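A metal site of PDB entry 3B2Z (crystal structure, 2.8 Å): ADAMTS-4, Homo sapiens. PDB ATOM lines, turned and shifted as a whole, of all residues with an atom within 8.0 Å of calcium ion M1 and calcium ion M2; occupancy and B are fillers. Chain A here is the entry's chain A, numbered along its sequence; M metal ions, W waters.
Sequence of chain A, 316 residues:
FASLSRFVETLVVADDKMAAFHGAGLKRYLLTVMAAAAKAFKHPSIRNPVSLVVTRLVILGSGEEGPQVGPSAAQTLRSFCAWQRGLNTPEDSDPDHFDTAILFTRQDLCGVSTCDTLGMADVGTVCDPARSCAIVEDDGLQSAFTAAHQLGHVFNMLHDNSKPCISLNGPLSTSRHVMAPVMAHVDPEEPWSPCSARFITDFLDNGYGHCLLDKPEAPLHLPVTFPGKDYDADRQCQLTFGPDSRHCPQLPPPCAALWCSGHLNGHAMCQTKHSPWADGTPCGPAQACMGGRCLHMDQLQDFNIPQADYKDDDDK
Calcium ion M1 is bound by OD1 of Asp 92 (2.3 Å), OD2 of Asp 214 (2.4 Å), O of Asp 92 (2.6 Å), OE1 of Glu 9 (2.6 Å) and OE2 of Glu 9 (2.8 Å). Calcium ion M1 has five donor atoms within binding distance.
Calcium ion M2 is bound by O of Cys 211 (2.3 Å). OD2 of Asp 99 is bound to calcium ion M2, at 2.3 Å. OD1 of Asp 214 is bound to calcium ion M2, at 2.5 Å. The side-chain carboxylate (OD2) of Asp 92 binds calcium ion M2 (2.5 Å). OE1 of Glu 9 binds calcium ion M2. OD1 of Asp 99 is bound to calcium ion M2, 2.5 Å away. Water W1 binds calcium ion M2, at 2.6 Å.
Water W1 lies within hydrogen-bond range of O of Asp 214 (2.5 Å) and O of Phe 7 (2.7 Å).
Within 4 Å of calcium ion M2: Glu 9, Asp 92, Asp 99, Cys 211 and Asp 214.
Residues that only touch calcium ion M1: His 97. Of the 27 residues printed, 4 come within 4 Å of calcium ion M1.
SG of Cys 127 is disulfide-bonded to SG of Cys 211. The backbone carbonyl oxygen (O) of Glu 9 sits at hydrogen-bond distance from the backbone NH (N) of Thr 100 (3.3 Å). ND1 of His 97 lies within hydrogen-bond range of O of Thr 89.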
ATOM      1  N   PHE A   7       2.403   1.240 -26.441  1.00  0.00           N
ATOM      2  CA  PHE A   7       3.768   1.316 -26.939  1.00  0.00           C
ATOM      3  C   PHE A   7       4.726   0.919 -25.817  1.00  0.00           C
ATOM      4  O   PHE A   7       4.636   1.440 -24.710  1.00  0.00           O
ATOM      5  CB  PHE A   7       4.100   2.724 -27.434  1.00  0.00           C
ATOM      6  CG  PHE A   7       3.220   3.224 -28.542  1.00  0.00           C
ATOM      7  CD1 PHE A   7       2.029   3.898 -28.263  1.00  0.00           C
ATOM      8  CD2 PHE A   7       3.585   3.037 -29.880  1.00  0.00           C
ATOM      9  CE1 PHE A   7       1.212   4.361 -29.291  1.00  0.00           C
ATOM     10  CE2 PHE A   7       2.769   3.503 -30.921  1.00  0.00           C
ATOM     11  CZ  PHE A   7       1.578   4.161 -30.618  1.00  0.00           C
ATOM     12  N   VAL A   8       5.629  -0.016 -26.089  1.00  0.00           N
ATOM     13  CA  VAL A   8       6.598  -0.417 -25.084  1.00  0.00           C
ATOM     14  C   VAL A   8       7.936   0.210 -25.409  1.00  0.00           C
ATOM     15  O   VAL A   8       8.611  -0.218 -26.340  1.00  0.00           O
ATOM     16  CB  VAL A   8       6.711  -1.948 -24.988  1.00  0.00           C
ATOM     17  CG1 VAL A   8       7.699  -2.336 -23.911  1.00  0.00           C
ATOM     18  CG2 VAL A   8       5.342  -2.562 -24.679  1.00  0.00           C
ATOM     19  N   GLU A   9       8.286   1.249 -24.656  1.00  0.00           N
ATOM     20  CA  GLU A   9       9.510   1.993 -24.907  1.00  0.00           C
ATOM     21  C   GLU A   9      10.666   1.183 -24.327  1.00  0.00           C
ATOM     22  O   GLU A   9      10.943   1.233 -23.123  1.00  0.00           O
ATOM     23  CB  GLU A   9       9.449   3.378 -24.254  1.00  0.00           C
ATOM     24  CG  GLU A   9       8.538   4.400 -24.953  1.00  0.00           C
ATOM     25  CD  GLU A   9       8.450   5.735 -24.205  1.00  0.00           C
ATOM     26  OE1 GLU A   9       7.774   5.834 -23.159  1.00  0.00           O
ATOM     27  OE2 GLU A   9       9.058   6.719 -24.676  1.00  0.00           O
ATOM     28  N   THR A  10      11.302   0.415 -25.204  1.00  0.00           N
ATOM     29  CA  THR A  10      12.294  -0.579 -24.817  1.00  0.00           C
ATOM     30  C   THR A  10      13.717  -0.036 -24.843  1.00  0.00           C
ATOM     31  O   THR A  10      14.144   0.563 -25.826  1.00  0.00           O
ATOM     32  CB  THR A  10      12.239  -1.784 -25.765  1.00  0.00           C
ATOM     33  OG1 THR A  10      10.874  -2.058 -26.097  1.00  0.00           O
ATOM     34  CG2 THR A  10      12.843  -3.017 -25.123  1.00  0.00           C
ATOM     35  N   THR A  55      13.732   2.544 -28.172  1.00  0.00           N
ATOM     36  CA  THR A  55      14.015   3.980 -28.099  1.00  0.00           C
ATOM     37  C   THR A  55      15.471   4.256 -27.769  1.00  0.00           C
ATOM     38  O   THR A  55      15.974   5.353 -28.026  1.00  0.00           O
ATOM     39  CB  THR A  55      13.107   4.736 -27.071  1.00  0.00           C
ATOM     40  OG1 THR A  55      13.406   4.298 -25.723  1.00  0.00           O
ATOM     41  CG2 THR A  55      11.631   4.521 -27.366  1.00  0.00           C
ATOM     42  N   THR A  89      14.849   7.319 -16.006  1.00  0.00           N
ATOM     43  CA  THR A  89      14.526   8.638 -15.448  1.00  0.00           C
ATOM     44  C   THR A  89      13.249   8.585 -14.586  1.00  0.00           C
ATOM     45  O   THR A  89      12.466   7.649 -14.716  1.00  0.00           O
ATOM     46  CB  THR A  89      14.357   9.704 -16.553  1.00  0.00           C
ATOM     47  OG1 THR A  89      13.371   9.249 -17.491  1.00  0.00           O
ATOM     48  CG2 THR A  89      15.674   9.959 -17.269  1.00  0.00           C
ATOM     49  N   GLU A  91      10.284  10.511 -14.556  1.00  0.00           N
ATOM     50  CA  GLU A  91       8.971  10.657 -15.201  1.00  0.00           C
ATOM     51  C   GLU A  91       9.028  10.277 -16.681  1.00  0.00           C
ATOM     52  O   GLU A  91       9.983  10.620 -17.371  1.00  0.00           O
ATOM     53  CB  GLU A  91       8.410  12.089 -15.043  1.00  0.00           C
ATOM     54  CG  GLU A  91       8.347  12.625 -13.591  1.00  0.00           C
ATOM     55  CD  GLU A  91       6.956  12.597 -12.944  1.00  0.00           C
ATOM     56  OE1 GLU A  91       6.247  11.555 -13.009  1.00  0.00           O
ATOM     57  OE2 GLU A  91       6.587  13.625 -12.326  1.00  0.00           O
ATOM     58  N   ASP A  92       7.979   9.597 -17.163  1.00  0.00           N
ATOM     59  CA  ASP A  92       7.890   9.088 -18.547  1.00  0.00           C
ATOM     60  C   ASP A  92       7.812  10.209 -19.597  1.00  0.00           C
ATOM     61  O   ASP A  92       7.455   9.979 -20.762  1.00  0.00           O
ATOM     62  CB  ASP A  92       6.681   8.159 -18.687  1.00  0.00           C
ATOM     63  CG  ASP A  92       6.832   7.145 -19.823  1.00  0.00           C
ATOM     64  OD1 ASP A  92       7.789   7.230 -20.623  1.00  0.00           O
ATOM     65  OD2 ASP A  92       5.963   6.248 -19.932  1.00  0.00           O
ATOM     66  N   SER A  93       8.146  11.418 -19.171  1.00  0.00           N
ATOM     67  CA  SER A  93       8.073  12.622 -19.984  1.00  0.00           C
ATOM     68  C   SER A  93       9.387  12.909 -20.701  1.00  0.00           C
ATOM     69  O   SER A  93       9.403  13.574 -21.743  1.00  0.00           O
ATOM     70  CB  SER A  93       7.728  13.787 -19.086  1.00  0.00           C
ATOM     71  OG  SER A  93       8.476  13.738 -17.873  1.00  0.00           O
ATOM     72  N   ASP A  94      10.480  12.414 -20.130  1.00  0.00           N
ATOM     73  CA  ASP A  94      11.809  12.529 -20.726  1.00  0.00           C
ATOM     74  C   ASP A  94      11.990  11.447 -21.794  1.00  0.00           C
ATOM     75  O   ASP A  94      11.834  10.266 -21.505  1.00  0.00           O
ATOM     76  CB  ASP A  94      12.888  12.412 -19.641  1.00  0.00           C
ATOM     77  CG  ASP A  94      14.288  12.783 -20.140  1.00  0.00           C
ATOM     78  OD1 ASP A  94      14.700  12.299 -21.217  1.00  0.00           O
ATOM     79  OD2 ASP A  94      14.994  13.552 -19.438  1.00  0.00           O
ATOM     80  N   PRO A  95      12.321  11.856 -23.029  1.00  0.00           N
ATOM     81  CA  PRO A  95      12.610  10.914 -24.106  1.00  0.00           C
ATOM     82  C   PRO A  95      13.526   9.755 -23.684  1.00  0.00           C
ATOM     83  O   PRO A  95      13.443   8.671 -24.265  1.00  0.00           O
ATOM     84  CB  PRO A  95      13.312  11.779 -25.146  1.00  0.00           C
ATOM     85  CG  PRO A  95      12.764  13.142 -24.945  1.00  0.00           C
ATOM     86  CD  PRO A  95      12.431  13.260 -23.480  1.00  0.00           C
ATOM     87  N   ASP A  96      14.398   9.996 -22.705  1.00  0.00           N
ATOM     88  CA  ASP A  96      15.307   8.968 -22.198  1.00  0.00           C
ATOM     89  C   ASP A  96      14.602   7.892 -21.352  1.00  0.00           C
ATOM     90  O   ASP A  96      15.150   6.808 -21.165  1.00  0.00           O
ATOM     91  CB  ASP A  96      16.453   9.609 -21.404  1.00  0.00           C
ATOM     92  CG  ASP A  96      17.518  10.263 -22.295  1.00  0.00           C
ATOM     93  OD1 ASP A  96      17.651   9.873 -23.488  1.00  0.00           O
ATOM     94  OD2 ASP A  96      18.237  11.155 -21.803  1.00  0.00           O
ATOM     95  N   HIS A  97      13.411   8.184 -20.847  1.00  0.00           N
ATOM     96  CA  HIS A  97      12.680   7.218 -20.050  1.00  0.00           C
ATOM     97  C   HIS A  97      12.240   6.035 -20.903  1.00  0.00           C
ATOM     98  O   HIS A  97      11.600   6.218 -21.942  1.00  0.00           O
ATOM     99  CB  HIS A  97      11.453   7.828 -19.366  1.00  0.00           C
ATOM    100  CG  HIS A  97      10.812   6.918 -18.366  1.00  0.00           C
ATOM    101  ND1 HIS A  97      10.932   6.849 -17.022  1.00  0.00           N
ATOM    102  CD2 HIS A  97       9.966   5.886 -18.727  1.00  0.00           C
ATOM    103  CE1 HIS A  97      10.150   5.799 -16.598  1.00  0.00           C
ATOM    104  NE2 HIS A  97       9.580   5.239 -17.648  1.00  0.00           N
ATOM    105  N   PHE A  98      12.584   4.842 -20.448  1.00  0.00           N
ATOM    106  CA  PHE A  98      12.161   3.631 -21.129  1.00  0.00           C
ATOM    107  C   PHE A  98      11.240   2.818 -20.207  1.00  0.00           C
ATOM    108  O   PHE A  98      11.321   2.921 -18.979  1.00  0.00           O
ATOM    109  CB  PHE A  98      13.379   2.808 -21.589  1.00  0.00           C
ATOM    110  CG  PHE A  98      14.377   2.541 -20.501  1.00  0.00           C
ATOM    111  CD1 PHE A  98      14.192   1.498 -19.615  1.00  0.00           C
ATOM    112  CD2 PHE A  98      15.509   3.333 -20.362  1.00  0.00           C
ATOM    113  CE1 PHE A  98      15.101   1.243 -18.587  1.00  0.00           C
ATOM    114  CE2 PHE A  98      16.435   3.096 -19.336  1.00  0.00           C
ATOM    115  CZ  PHE A  98      16.229   2.044 -18.447  1.00  0.00           C
ATOM    116  N   ASP A  99      10.363   2.021 -20.814  1.00  0.00           N
ATOM    117  CA  ASP A  99       9.391   1.205 -20.077  1.00  0.00           C
ATOM    118  C   ASP A  99       9.932  -0.161 -19.639  1.00  0.00           C
ATOM    119  O   ASP A  99       9.660  -0.599 -18.529  1.00  0.00           O
ATOM    120  CB  ASP A  99       8.106   1.041 -20.907  1.00  0.00           C
ATOM    121  CG  ASP A  99       7.399   2.373 -21.155  1.00  0.00           C
ATOM    122  OD1 ASP A  99       7.453   3.271 -20.301  1.00  0.00           O
ATOM    123  OD2 ASP A  99       6.761   2.518 -22.218  1.00  0.00           O
ATOM    124  N   THR A 100      10.672  -0.847 -20.518  1.00  0.00           N
ATOM    125  CA  THR A 100      11.350  -2.081 -20.109  1.00  0.00           C
ATOM    126  C   THR A 100      12.738  -2.192 -20.711  1.00  0.00           C
ATOM    127  O   THR A 100      13.038  -1.513 -21.683  1.00  0.00           O
ATOM    128  CB  THR A 100      10.558  -3.366 -20.409  1.00  0.00           C
ATOM    129  OG1 THR A 100      11.240  -4.493 -19.826  1.00  0.00           O
ATOM    130  CG2 THR A 100      10.368  -3.584 -21.910  1.00  0.00           C
ATOM    131  N   VAL A 126       5.631  -4.739 -16.264  1.00  0.00           N
ATOM    132  CA  VAL A 126       5.841  -3.796 -17.357  1.00  0.00           C
ATOM    133  C   VAL A 126       6.104  -2.371 -16.893  1.00  0.00           C
ATOM    134  O   VAL A 126       7.019  -1.722 -17.400  1.00  0.00           O
ATOM    135  CB  VAL A 126       4.666  -3.720 -18.362  1.00  0.00           C
ATOM    136  CG1 VAL A 126       5.214  -3.510 -19.773  1.00  0.00           C
ATOM    137  CG2 VAL A 126       3.833  -4.974 -18.306  1.00  0.00           C
ATOM    138  N   CYS A 127       5.291  -1.899 -15.953  1.00  0.00           N
ATOM    139  CA  CYS A 127       5.351  -0.498 -15.530  1.00  0.00           C
ATOM    140  C   CYS A 127       5.928  -0.255 -14.140  1.00  0.00           C
ATOM    141  O   CYS A 127       5.767   0.818 -13.572  1.00  0.00           O
ATOM    142  CB  CYS A 127       3.987   0.176 -15.716  1.00  0.00           C
ATOM    143  SG  CYS A 127       3.520   0.340 -17.458  1.00  0.00           S
ATOM    144  N   GLY A 209      -0.797  -1.540 -17.517  1.00  0.00           N
ATOM    145  CA  GLY A 209      -0.040  -0.927 -18.607  1.00  0.00           C
ATOM    146  C   GLY A 209      -0.359   0.552 -18.765  1.00  0.00           C
ATOM    147  O   GLY A 209      -0.631   1.005 -19.878  1.00  0.00           O
ATOM    148  N   HIS A 210      -0.321   1.280 -17.647  1.00  0.00           N
ATOM    149  CA  HIS A 210      -0.643   2.706 -17.607  1.00  0.00           C
ATOM    150  C   HIS A 210       0.467   3.545 -18.209  1.00  0.00           C
ATOM    151  O   HIS A 210       0.259   4.705 -18.574  1.00  0.00           O
ATOM    152  CB  HIS A 210      -0.894   3.153 -16.165  1.00  0.00           C
ATOM    153  CG  HIS A 210       0.343   3.313 -15.349  1.00  0.00           C
ATOM    154  ND1 HIS A 210       0.870   2.294 -14.568  1.00  0.00           N
ATOM    155  CD2 HIS A 210       1.165   4.373 -15.169  1.00  0.00           C
ATOM    156  CE1 HIS A 210       1.954   2.731 -13.952  1.00  0.00           C
ATOM    157  NE2 HIS A 210       2.159   3.987 -14.303  1.00  0.00           N
ATOM    158  N   CYS A 211       1.648   2.950 -18.314  1.00  0.00           N
ATOM    159  CA  CYS A 211       2.841   3.683 -18.727  1.00  0.00           C
ATOM    160  C   CYS A 211       3.182   3.429 -20.203  1.00  0.00           C
ATOM    161  O   CYS A 211       4.168   3.945 -20.728  1.00  0.00           O
ATOM    162  CB  CYS A 211       4.006   3.315 -17.798  1.00  0.00           C
ATOM    163  SG  CYS A 211       4.795   1.752 -18.179  1.00  0.00           S
ATOM    164  N   LEU A 212       2.342   2.645 -20.860  1.00  0.00           N
ATOM    165  CA  LEU A 212       2.566   2.297 -22.251  1.00  0.00           C
ATOM    166  C   LEU A 212       1.687   3.124 -23.157  1.00  0.00           C
ATOM    167  O   LEU A 212       1.428   2.741 -24.297  1.00  0.00           O
ATOM    168  CB  LEU A 212       2.237   0.819 -22.472  1.00  0.00           C
ATOM    169  CG  LEU A 212       2.749  -0.234 -21.495  1.00  0.00           C
ATOM    170  CD1 LEU A 212       2.247  -1.594 -21.967  1.00  0.00           C
ATOM    171  CD2 LEU A 212       4.267  -0.202 -21.403  1.00  0.00           C
ATOM    172  N   LEU A 213       1.227   4.273 -22.653  1.00  0.00           N
ATOM    173  CA  LEU A 213       0.249   5.061 -23.392  1.00  0.00           C
ATOM    174  C   LEU A 213       0.871   6.230 -24.100  1.00  0.00           C
ATOM    175  O   LEU A 213       0.336   6.667 -25.127  1.00  0.00           O
ATOM    176  CB  LEU A 213      -0.891   5.519 -22.492  1.00  0.00           C
ATOM    177  CG  LEU A 213      -2.106   4.577 -22.371  1.00  0.00           C
ATOM    178  CD1 LEU A 213      -3.160   5.207 -21.468  1.00  0.00           C
ATOM    179  CD2 LEU A 213      -2.695   4.260 -23.737  1.00  0.00           C
ATOM    180  N   ASP A 214       1.993   6.735 -23.587  1.00  0.00           N
ATOM    181  CA  ASP A 214       2.762   7.771 -24.280  1.00  0.00           C
ATOM    182  C   ASP A 214       3.559   7.201 -25.460  1.00  0.00           C
ATOM    183  O   ASP A 214       4.202   6.157 -25.354  1.00  0.00           O
ATOM    184  CB  ASP A 214       3.658   8.579 -23.323  1.00  0.00           C
ATOM    185  CG  ASP A 214       4.909   7.836 -22.897  1.00  0.00           C
ATOM    186  OD1 ASP A 214       4.788   6.753 -22.284  1.00  0.00           O
ATOM    187  OD2 ASP A 214       6.019   8.335 -23.167  1.00  0.00           O
ATOM    188  N   LYS A 215       3.485   7.894 -26.588  1.00  0.00           N
ATOM    189  CA  LYS A 215       4.219   7.513 -27.794  1.00  0.00           C
ATOM    190  C   LYS A 215       5.586   8.209 -27.825  1.00  0.00           C
ATOM    191  O   LYS A 215       5.638   9.445 -27.717  1.00  0.00           O
ATOM    192  CB  LYS A 215       3.383   7.849 -29.034  1.00  0.00           C
ATOM    193  CG  LYS A 215       3.933   7.312 -30.348  1.00  0.00           C
ATOM    194  CD  LYS A 215       3.053   7.717 -31.524  1.00  0.00           C
ATOM    195  CE  LYS A 215       3.617   7.189 -32.849  1.00  0.00           C
ATOM    196  NZ  LYS A 215       2.693   7.430 -33.999  1.00  0.00           N
ATOM    197  N   PRO A 216       6.690   7.447 -27.991  1.00  0.00           N
ATOM    198  CA  PRO A 216       8.009   8.063 -28.033  1.00  0.00           C
ATOM    199  C   PRO A 216       8.197   8.854 -29.323  1.00  0.00           C
ATOM    200  O   PRO A 216       7.762   8.401 -30.386  1.00  0.00           O
ATOM    201  CB  PRO A 216       8.955   6.860 -28.030  1.00  0.00           C
ATOM    202  CG  PRO A 216       8.176   5.763 -28.641  1.00  0.00           C
ATOM    203  CD  PRO A 216       6.765   5.979 -28.163  1.00  0.00           C
ATOM    204  N   GLU A 217       8.830  10.013 -29.223  1.00  0.00           N
ATOM    205  CA  GLU A 217       8.995  10.870 -30.402  1.00  0.00           C
ATOM    206  C   GLU A 217       9.950  10.287 -31.447  1.00  0.00           C
ATOM    207  O   GLU A 217       9.659  10.337 -32.635  1.00  0.00           O
ATOM    208  CB  GLU A 217       9.375  12.293 -29.982  1.00  0.00           C
ATOM    209  CG  GLU A 217       8.221  13.033 -29.270  1.00  0.00           C
ATOM    210  CD  GLU A 217       8.654  14.185 -28.338  1.00  0.00           C
ATOM    211  OE1 GLU A 217       9.870  14.451 -28.182  1.00  0.00           O
ATOM    212  OE2 GLU A 217       7.745  14.815 -27.753  1.00  0.00           O
HETATM  213 CA    CA M   1       8.344   8.341 -22.547  1.00  0.00          CA
HETATM  214 CA    CA M   2       6.035   4.680 -21.837  1.00  0.00          CA
HETATM  215  O   HOH W   1       4.817   4.093 -24.032  1.00  0.00           O
